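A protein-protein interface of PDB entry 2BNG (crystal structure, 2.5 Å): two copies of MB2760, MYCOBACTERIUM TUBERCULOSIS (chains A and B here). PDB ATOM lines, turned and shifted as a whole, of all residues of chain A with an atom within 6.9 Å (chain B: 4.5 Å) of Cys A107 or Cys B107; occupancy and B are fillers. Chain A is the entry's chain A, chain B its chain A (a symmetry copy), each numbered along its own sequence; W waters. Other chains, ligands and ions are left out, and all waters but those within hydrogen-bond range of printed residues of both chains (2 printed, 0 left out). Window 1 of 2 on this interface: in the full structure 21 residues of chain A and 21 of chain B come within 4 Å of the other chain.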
ATOM      1  N   VAL A  49     -26.572 -11.707   8.917  1.00  0.00           N
ATOM      2  CA  VAL A  49     -25.187 -11.220   9.014  1.00  0.00           C
ATOM      3  C   VAL A  49     -24.137 -12.230   8.618  1.00  0.00           C
ATOM      4  O   VAL A  49     -24.212 -13.431   8.940  1.00  0.00           O
ATOM      5  CB  VAL A  49     -24.845 -10.240  10.206  1.00  0.00           C
ATOM      6  CG1 VAL A  49     -25.925 -10.053  11.094  1.00  0.00           C
ATOM      7  CG2 VAL A  49     -23.700 -10.663  10.970  1.00  0.00           C
ATOM      8  N   LEU A  88     -34.435  -5.253  20.085  1.00  0.00           N
ATOM      9  CA  LEU A  88     -33.582  -6.430  20.006  1.00  0.00           C
ATOM     10  C   LEU A  88     -34.387  -7.630  20.458  1.00  0.00           C
ATOM     11  O   LEU A  88     -35.225  -7.502  21.344  1.00  0.00           O
ATOM     12  CB  LEU A  88     -32.317  -6.271  20.856  1.00  0.00           C
ATOM     13  CG  LEU A  88     -31.341  -5.114  20.570  1.00  0.00           C
ATOM     14  CD1 LEU A  88     -31.724  -3.825  21.303  1.00  0.00           C
ATOM     15  CD2 LEU A  88     -29.913  -5.509  20.958  1.00  0.00           C
ATOM     16  N   THR A  89     -34.119  -8.783  19.836  1.00  0.00           N
ATOM     17  CA  THR A  89     -34.822 -10.024  20.140  1.00  0.00           C
ATOM     18  C   THR A  89     -33.863 -11.189  20.368  1.00  0.00           C
ATOM     19  O   THR A  89     -32.861 -11.294  19.676  1.00  0.00           O
ATOM     20  CB  THR A  89     -35.774 -10.447  18.992  1.00  0.00           C
ATOM     21  OG1 THR A  89     -35.066 -10.567  17.762  1.00  0.00           O
ATOM     22  CG2 THR A  89     -36.784  -9.470  18.759  1.00  0.00           C
ATOM     23  N   GLU A  90     -34.183 -12.058  21.326  1.00  0.00           N
ATOM     24  CA  GLU A  90     -33.538 -13.359  21.461  1.00  0.00           C
ATOM     25  C   GLU A  90     -34.581 -14.410  21.080  1.00  0.00           C
ATOM     26  O   GLU A  90     -35.635 -14.513  21.750  1.00  0.00           O
ATOM     27  CB  GLU A  90     -33.061 -13.590  22.899  1.00  0.00           C
ATOM     28  CG  GLU A  90     -32.448 -14.962  23.136  1.00  0.00           C
ATOM     29  CD  GLU A  90     -32.225 -15.327  24.617  1.00  0.00           C
ATOM     30  OE1 GLU A  90     -33.007 -14.892  25.506  1.00  0.00           O
ATOM     31  OE2 GLU A  90     -31.270 -16.089  24.886  1.00  0.00           O
ATOM     32  N   ARG A  91     -34.285 -15.200  20.043  1.00  0.00           N
ATOM     33  CA  ARG A  91     -35.283 -16.109  19.471  1.00  0.00           C
ATOM     34  C   ARG A  91     -34.743 -17.487  19.189  1.00  0.00           C
ATOM     35  O   ARG A  91     -33.521 -17.704  19.203  1.00  0.00           O
ATOM     36  CB  ARG A  91     -35.853 -15.569  18.148  1.00  0.00           C
ATOM     37  CG  ARG A  91     -35.818 -14.066  17.987  1.00  0.00           C
ATOM     38  CD  ARG A  91     -36.675 -13.570  16.880  1.00  0.00           C
ATOM     39  NE  ARG A  91     -36.324 -14.088  15.559  1.00  0.00           N
ATOM     40  CZ  ARG A  91     -35.689 -13.382  14.624  1.00  0.00           C
ATOM     41  NH1 ARG A  91     -35.316 -12.142  14.883  1.00  0.00           N
ATOM     42  NH2 ARG A  91     -35.436 -13.905  13.431  1.00  0.00           N
ATOM     43  N   TRP A 105     -30.862 -20.910  16.975  1.00  0.00           N
ATOM     44  CA  TRP A 105     -31.060 -19.634  17.645  1.00  0.00           C
ATOM     45  C   TRP A 105     -30.843 -18.456  16.700  1.00  0.00           C
ATOM     46  O   TRP A 105     -30.017 -18.535  15.779  1.00  0.00           O
ATOM     47  CB  TRP A 105     -30.202 -19.497  18.906  1.00  0.00           C
ATOM     48  CG  TRP A 105     -28.719 -19.527  18.740  1.00  0.00           C
ATOM     49  CD1 TRP A 105     -27.889 -20.572  19.037  1.00  0.00           C
ATOM     50  CD2 TRP A 105     -27.857 -18.440  18.336  1.00  0.00           C
ATOM     51  NE1 TRP A 105     -26.570 -20.223  18.807  1.00  0.00           N
ATOM     52  CE2 TRP A 105     -26.520 -18.919  18.391  1.00  0.00           C
ATOM     53  CE3 TRP A 105     -28.080 -17.100  17.943  1.00  0.00           C
ATOM     54  CZ2 TRP A 105     -25.408 -18.110  18.065  1.00  0.00           C
ATOM     55  CZ3 TRP A 105     -26.966 -16.298  17.595  1.00  0.00           C
ATOM     56  CH2 TRP A 105     -25.652 -16.811  17.664  1.00  0.00           C
ATOM     57  N   VAL A 106     -31.605 -17.379  16.914  1.00  0.00           N
ATOM     58  CA  VAL A 106     -31.382 -16.136  16.200  1.00  0.00           C
ATOM     59  C   VAL A 106     -31.465 -14.975  17.162  1.00  0.00           C
ATOM     60  O   VAL A 106     -32.348 -14.950  18.031  1.00  0.00           O
ATOM     61  CB  VAL A 106     -32.403 -15.935  15.044  1.00  0.00           C
ATOM     62  CG1 VAL A 106     -32.185 -14.580  14.366  1.00  0.00           C
ATOM     63  CG2 VAL A 106     -32.255 -17.020  14.017  1.00  0.00           C
ATOM     64  N   CYS A 107     -30.525 -14.034  17.060  1.00  0.00           N
ATOM     65  CA  CYS A 107     -30.714 -12.731  17.718  1.00  0.00           C
ATOM     66  C   CYS A 107     -30.973 -11.718  16.615  1.00  0.00           C
ATOM     67  O   CYS A 107     -30.142 -11.542  15.701  1.00  0.00           O
ATOM     68  CB  CYS A 107     -29.515 -12.320  18.553  1.00  0.00           C
ATOM     69  SG  CYS A 107     -29.211 -13.349  19.986  1.00  0.00           S
ATOM     70  N   GLY A 108     -32.138 -11.087  16.666  1.00  0.00           N
ATOM     71  CA  GLY A 108     -32.515 -10.140  15.634  1.00  0.00           C
ATOM     72  C   GLY A 108     -32.529  -8.731  16.187  1.00  0.00           C
ATOM     73  O   GLY A 108     -33.086  -8.501  17.275  1.00  0.00           O
ATOM     74  N   VAL A 109     -31.906  -7.803  15.452  1.00  0.00           N
ATOM     75  CA  VAL A 109     -32.021  -6.388  15.772  1.00  0.00           C
ATOM     76  C   VAL A 109     -32.815  -5.618  14.711  1.00  0.00           C
ATOM     77  O   VAL A 109     -32.643  -5.828  13.521  1.00  0.00           O
ATOM     78  CB  VAL A 109     -30.665  -5.703  16.227  1.00  0.00           C
ATOM     79  CG1 VAL A 109     -29.621  -6.712  16.592  1.00  0.00           C
ATOM     80  CG2 VAL A 109     -30.146  -4.682  15.227  1.00  0.00           C
ATOM     81  N   PHE A 110     -33.727  -4.770  15.176  1.00  0.00           N
ATOM     82  CA  PHE A 110     -34.640  -4.089  14.282  1.00  0.00           C
ATOM     83  C   PHE A 110     -34.583  -2.607  14.547  1.00  0.00           C
ATOM     84  O   PHE A 110     -34.238  -2.163  15.648  1.00  0.00           O
ATOM     85  CB  PHE A 110     -36.086  -4.581  14.477  1.00  0.00           C
ATOM     86  CG  PHE A 110     -36.281  -6.068  14.240  1.00  0.00           C
ATOM     87  CD1 PHE A 110     -35.973  -6.978  15.220  1.00  0.00           C
ATOM     88  CD2 PHE A 110     -36.792  -6.534  13.055  1.00  0.00           C
ATOM     89  CE1 PHE A 110     -36.161  -8.312  15.033  1.00  0.00           C
ATOM     90  CE2 PHE A 110     -36.985  -7.894  12.857  1.00  0.00           C
ATOM     91  CZ  PHE A 110     -36.682  -8.780  13.854  1.00  0.00           C
ATOM     92  N   ARG A 121     -32.057  -7.110  11.129  1.00  0.00           N
ATOM     93  CA  ARG A 121     -30.747  -7.716  11.129  1.00  0.00           C
ATOM     94  C   ARG A 121     -30.716  -8.976  11.969  1.00  0.00           C
ATOM     95  O   ARG A 121     -30.744  -8.902  13.196  1.00  0.00           O
ATOM     96  CB  ARG A 121     -29.699  -6.715  11.599  1.00  0.00           C
ATOM     97  CG  ARG A 121     -28.277  -7.239  11.544  1.00  0.00           C
ATOM     98  CD  ARG A 121     -27.284  -6.236  12.083  1.00  0.00           C
ATOM     99  NE  ARG A 121     -27.151  -5.070  11.221  1.00  0.00           N
ATOM    100  CZ  ARG A 121     -26.920  -3.829  11.667  1.00  0.00           C
ATOM    101  NH1 ARG A 121     -26.836  -3.557  12.976  1.00  0.00           N
ATOM    102  NH2 ARG A 121     -26.799  -2.847  10.791  1.00  0.00           N
ATOM    103  N   ASP A 122     -30.667 -10.136  11.304  1.00  0.00           N
ATOM    104  CA  ASP A 122     -30.617 -11.406  12.015  1.00  0.00           C
ATOM    105  C   ASP A 122     -29.182 -11.960  12.130  1.00  0.00           C
ATOM    106  O   ASP A 122     -28.445 -12.039  11.144  1.00  0.00           O
ATOM    107  CB  ASP A 122     -31.541 -12.434  11.366  1.00  0.00           C
ATOM    108  CG  ASP A 122     -33.017 -12.259  11.765  1.00  0.00           C
ATOM    109  OD1 ASP A 122     -33.379 -11.501  12.712  1.00  0.00           O
ATOM    110  OD2 ASP A 122     -33.842 -12.931  11.121  1.00  0.00           O
ATOM    111  N   TYR A 123     -28.816 -12.317  13.362  1.00  0.00           N
ATOM    112  CA  TYR A 123     -27.566 -12.933  13.710  1.00  0.00           C
ATOM    113  C   TYR A 123     -27.832 -14.370  14.096  1.00  0.00           C
ATOM    114  O   TYR A 123     -28.767 -14.649  14.848  1.00  0.00           O
ATOM    115  CB  TYR A 123     -27.010 -12.278  14.968  1.00  0.00           C
ATOM    116  CG  TYR A 123     -26.518 -10.871  14.838  1.00  0.00           C
ATOM    117  CD1 TYR A 123     -27.383  -9.793  14.979  1.00  0.00           C
ATOM    118  CD2 TYR A 123     -25.171 -10.615  14.618  1.00  0.00           C
ATOM    119  CE1 TYR A 123     -26.907  -8.485  14.906  1.00  0.00           C
ATOM    120  CE2 TYR A 123     -24.693  -9.320  14.525  1.00  0.00           C
ATOM    121  CZ  TYR A 123     -25.563  -8.265  14.666  1.00  0.00           C
ATOM    122  OH  TYR A 123     -25.063  -6.990  14.599  1.00  0.00           O
ATOM    123  N   PHE A 124     -26.975 -15.267  13.620  1.00  0.00           N
ATOM    124  CA  PHE A 124     -27.005 -16.664  13.975  1.00  0.00           C
ATOM    125  C   PHE A 124     -25.618 -17.249  13.752  1.00  0.00           C
ATOM    126  O   PHE A 124     -24.735 -16.582  13.209  1.00  0.00           O
ATOM    127  CB  PHE A 124     -28.036 -17.396  13.113  1.00  0.00           C
ATOM    128  CG  PHE A 124     -27.917 -17.086  11.662  1.00  0.00           C
ATOM    129  CD1 PHE A 124     -28.721 -16.103  11.082  1.00  0.00           C
ATOM    130  CD2 PHE A 124     -26.989 -17.759  10.864  1.00  0.00           C
ATOM    131  CE1 PHE A 124     -28.609 -15.798   9.720  1.00  0.00           C
ATOM    132  CE2 PHE A 124     -26.870 -17.475   9.512  1.00  0.00           C
ATOM    133  CZ  PHE A 124     -27.678 -16.488   8.936  1.00  0.00           C
ATOM    134  N   THR B  89     -28.033  -6.753  24.114  1.00  0.00           N
ATOM    135  CA  THR B  89     -26.993  -5.918  23.524  1.00  0.00           C
ATOM    136  C   THR B  89     -26.586  -6.401  22.134  1.00  0.00           C
ATOM    137  O   THR B  89     -26.508  -7.600  21.908  1.00  0.00           O
ATOM    138  CB  THR B  89     -25.705  -5.901  24.386  1.00  0.00           C
ATOM    139  OG1 THR B  89     -25.218  -7.223  24.600  1.00  0.00           O
ATOM    140  CG2 THR B  89     -25.947  -5.367  25.684  1.00  0.00           C
ATOM    141  N   TRP B 105     -18.503 -10.052  16.105  1.00  0.00           N
ATOM    142  CA  TRP B 105     -19.757  -9.577  16.670  1.00  0.00           C
ATOM    143  C   TRP B 105     -20.226 -10.451  17.829  1.00  0.00           C
ATOM    144  O   TRP B 105     -19.979 -11.666  17.838  1.00  0.00           O
ATOM    145  CB  TRP B 105     -20.853  -9.426  15.611  1.00  0.00           C
ATOM    146  CG  TRP B 105     -21.291 -10.657  14.889  1.00  0.00           C
ATOM    147  CD1 TRP B 105     -20.964 -11.007  13.609  1.00  0.00           C
ATOM    148  CD2 TRP B 105     -22.219 -11.663  15.350  1.00  0.00           C
ATOM    149  NE1 TRP B 105     -21.596 -12.187  13.254  1.00  0.00           N
ATOM    150  CE2 TRP B 105     -22.381 -12.603  14.295  1.00  0.00           C
ATOM    151  CE3 TRP B 105     -22.945 -11.860  16.548  1.00  0.00           C
ATOM    152  CZ2 TRP B 105     -23.233 -13.725  14.401  1.00  0.00           C
ATOM    153  CZ3 TRP B 105     -23.780 -12.998  16.660  1.00  0.00           C
ATOM    154  CH2 TRP B 105     -23.913 -13.908  15.588  1.00  0.00           C
ATOM    155  N   VAL B 106     -20.875  -9.824  18.815  1.00  0.00           N
ATOM    156  CA  VAL B 106     -21.520 -10.559  19.888  1.00  0.00           C
ATOM    157  C   VAL B 106     -22.885  -9.973  20.157  1.00  0.00           C
ATOM    158  O   VAL B 106     -23.042  -8.744  20.171  1.00  0.00           O
ATOM    159  CB  VAL B 106     -20.675 -10.547  21.194  1.00  0.00           C
ATOM    160  CG1 VAL B 106     -21.422 -11.264  22.322  1.00  0.00           C
ATOM    161  CG2 VAL B 106     -19.357 -11.231  20.974  1.00  0.00           C
ATOM    162  N   CYS B 107     -23.894 -10.832  20.316  1.00  0.00           N
ATOM    163  CA  CYS B 107     -25.165 -10.373  20.900  1.00  0.00           C
ATOM    164  C   CYS B 107     -25.247 -10.974  22.294  1.00  0.00           C
ATOM    165  O   CYS B 107     -25.200 -12.209  22.461  1.00  0.00           O
ATOM    166  CB  CYS B 107     -26.368 -10.779  20.068  1.00  0.00           C
ATOM    167  SG  CYS B 107     -26.466  -9.998  18.460  1.00  0.00           S
ATOM    168  N   GLY B 108     -25.322 -10.108  23.297  1.00  0.00           N
ATOM    169  CA  GLY B 108     -25.349 -10.568  24.672  1.00  0.00           C
ATOM    170  C   GLY B 108     -26.710 -10.319  25.287  1.00  0.00           C
ATOM    171  O   GLY B 108     -27.259  -9.214  25.141  1.00  0.00           O
ATOM    172  N   VAL B 109     -27.252 -11.345  25.954  1.00  0.00           N
ATOM    173  CA  VAL B 109     -28.454 -11.170  26.754  1.00  0.00           C
ATOM    174  C   VAL B 109     -28.177 -11.317  28.254  1.00  0.00           C
ATOM    175  O   VAL B 109     -27.444 -12.198  28.675  1.00  0.00           O
ATOM    176  CB  VAL B 109     -29.721 -11.963  26.223  1.00  0.00           C
ATOM    177  CG1 VAL B 109     -29.537 -12.436  24.814  1.00  0.00           C
ATOM    178  CG2 VAL B 109     -30.153 -13.089  27.149  1.00  0.00           C
ATOM    179  N   ARG B 121     -25.409 -14.079  28.838  1.00  0.00           N
ATOM    180  CA  ARG B 121     -25.435 -15.022  27.746  1.00  0.00           C
ATOM    181  C   ARG B 121     -24.939 -14.398  26.459  1.00  0.00           C
ATOM    182  O   ARG B 121     -25.641 -13.591  25.852  1.00  0.00           O
ATOM    183  CB  ARG B 121     -26.835 -15.598  27.577  1.00  0.00           C
ATOM    184  CG  ARG B 121     -26.935 -16.670  26.506  1.00  0.00           C
ATOM    185  CD  ARG B 121     -28.352 -17.160  26.329  1.00  0.00           C
ATOM    186  NE  ARG B 121     -28.826 -17.916  27.480  1.00  0.00           N
ATOM    187  CZ  ARG B 121     -30.093 -17.907  27.914  1.00  0.00           C
ATOM    188  NH1 ARG B 121     -31.030 -17.149  27.332  1.00  0.00           N
ATOM    189  NH2 ARG B 121     -30.413 -18.647  28.961  1.00  0.00           N
ATOM    190  N   ASP B 122     -23.721 -14.767  26.046  1.00  0.00           N
ATOM    191  CA  ASP B 122     -23.156 -14.239  24.813  1.00  0.00           C
ATOM    192  C   ASP B 122     -23.329 -15.207  23.624  1.00  0.00           C
ATOM    193  O   ASP B 122     -23.014 -16.397  23.717  1.00  0.00           O
ATOM    194  CB  ASP B 122     -21.685 -13.870  24.997  1.00  0.00           C
ATOM    195  CG  ASP B 122     -21.485 -12.506  25.683  1.00  0.00           C
ATOM    196  OD1 ASP B 122     -22.433 -11.684  25.848  1.00  0.00           O
ATOM    197  OD2 ASP B 122     -20.324 -12.238  26.040  1.00  0.00           O
ATOM    198  N   TYR B 123     -23.852 -14.660  22.527  1.00  0.00           N
ATOM    199  CA  TYR B 123     -24.034 -15.333  21.271  1.00  0.00           C
ATOM    200  C   TYR B 123     -23.050 -14.761  20.276  1.00  0.00           C
ATOM    201  O   TYR B 123     -22.895 -13.542  20.186  1.00  0.00           O
ATOM    202  CB  TYR B 123     -25.411 -14.998  20.711  1.00  0.00           C
ATOM    203  CG  TYR B 123     -26.592 -15.574  21.425  1.00  0.00           C
ATOM    204  CD1 TYR B 123     -27.165 -14.917  22.507  1.00  0.00           C
ATOM    205  CD2 TYR B 123     -27.167 -16.761  20.990  1.00  0.00           C
ATOM    206  CE1 TYR B 123     -28.295 -15.435  23.137  1.00  0.00           C
ATOM    207  CE2 TYR B 123     -28.278 -17.292  21.621  1.00  0.00           C
ATOM    208  CZ  TYR B 123     -28.831 -16.629  22.691  1.00  0.00           C
ATOM    209  OH  TYR B 123     -29.950 -17.159  23.283  1.00  0.00           O
HETATM  210  O   HOH W   1     -21.693 -13.908  10.950  1.00  0.00           O
HETATM  211  O   HOH W   2     -32.300 -18.222  21.499  1.00  0.00           O
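Cys B107 touches just these residues of chain A: Cys A107 (3.8 Å) and Tyr A123 (3.6 Å). Of the printed residues of chain A, Val B109 touches Glu A90. Of the printed residues of chain A, Arg B121 touches Glu A90. Asp B122 touches none of the printed residues of chain A. Asp A122 touches none of the printed residues of chain B. The nearest printed residue of chain B that does not touch Cys A107 is Val B109 (4.9 Å).
Water W2 bridges O of Arg A91 (2.7 Å) and OH of Tyr B123 (3.1 Å). Water W1 bridges NE1 of Trp B105 (2.9 Å) and O of Val A49 (3.3 Å).
O of Asp A122 lies within hydrogen-bond range of N of Val A49 (2.9 Å). The backbone NH of Tyr A123 sits at hydrogen-bond distance from the backbone carbonyl oxygen of Cys A107, at 2.8 Å. The backbone NH (N) of Thr B89 sits at hydrogen-bond distance from the backbone carbonyl oxygen (O) of Gly B108. The backbone carbonyl oxygen (O) of Cys B107 lies within hydrogen-bond range of the backbone NH (N) of Tyr B123, 2.8 Å away. The backbone NH (N) of Val B109 is in hydrogen-bond range of the backbone carbonyl oxygen (O) of Arg B121 (2.8 Å).
The side-chain carboxylate (OE2) of Glu A90 is in salt-bridge range of the guanidinium group (NH1) of Arg B121, 2.7 Å away. OH of Tyr B123 sits close to OE2 of Glu A90, at 2.3 Å.
Val A49 touches Trp B105 (CG2 to NE1, 3.5 Å). Leu A88 touches Thr B89 (CD2 to C, 3.6 Å). OE1 of Glu A90 touches CG2 of Val B109 (3.8 Å). CH2 of Trp B105 touches CH2 of Trp A105 (3.97 Å). CD2 of Tyr B123 touches CE3 of Trp A105 (3.2 Å). CB of Cys B107 touches CB of Cys A107, 3.8 Å away. Tyr B123 touches Cys A107 (CD1 to SG, 3.6 Å). Tyr A123 touches Trp B105 (CD2 to CE3, 3.2 Å). Cys B107 touches Tyr A123 (SG to CD1, 3.6 Å). CZ2 of Trp B105 touches O of Phe A124, at 3.4 Å.
Of the 15 printed residues of chain A, 7 touch a printed residue of chain B. Hydrophobic or aromatic side chains of chain A within 4 Å of the printed part of chain B: Val A49, Leu A88, Trp A105 and Tyr A123. Among the printed residues, 12 pairs touch across the chains.
Trp A105 touches its own counterpart, Trp B105. Trp A105 touches Tyr B123, and with the chains exchanged Tyr A123 touches Trp B105. Cys B107 touches its own counterpart, Cys A107. Cys A107 touches Tyr B123, and with the chains exchanged Tyr A123 touches Cys B107. Positions printed for both chains: 89, 105, 106, 107, 108, 109, 121, 122 and 123. Of the 12 pairs that touch across the chains among the printed residues, 6 have their exchanged pair printed and touching as well.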
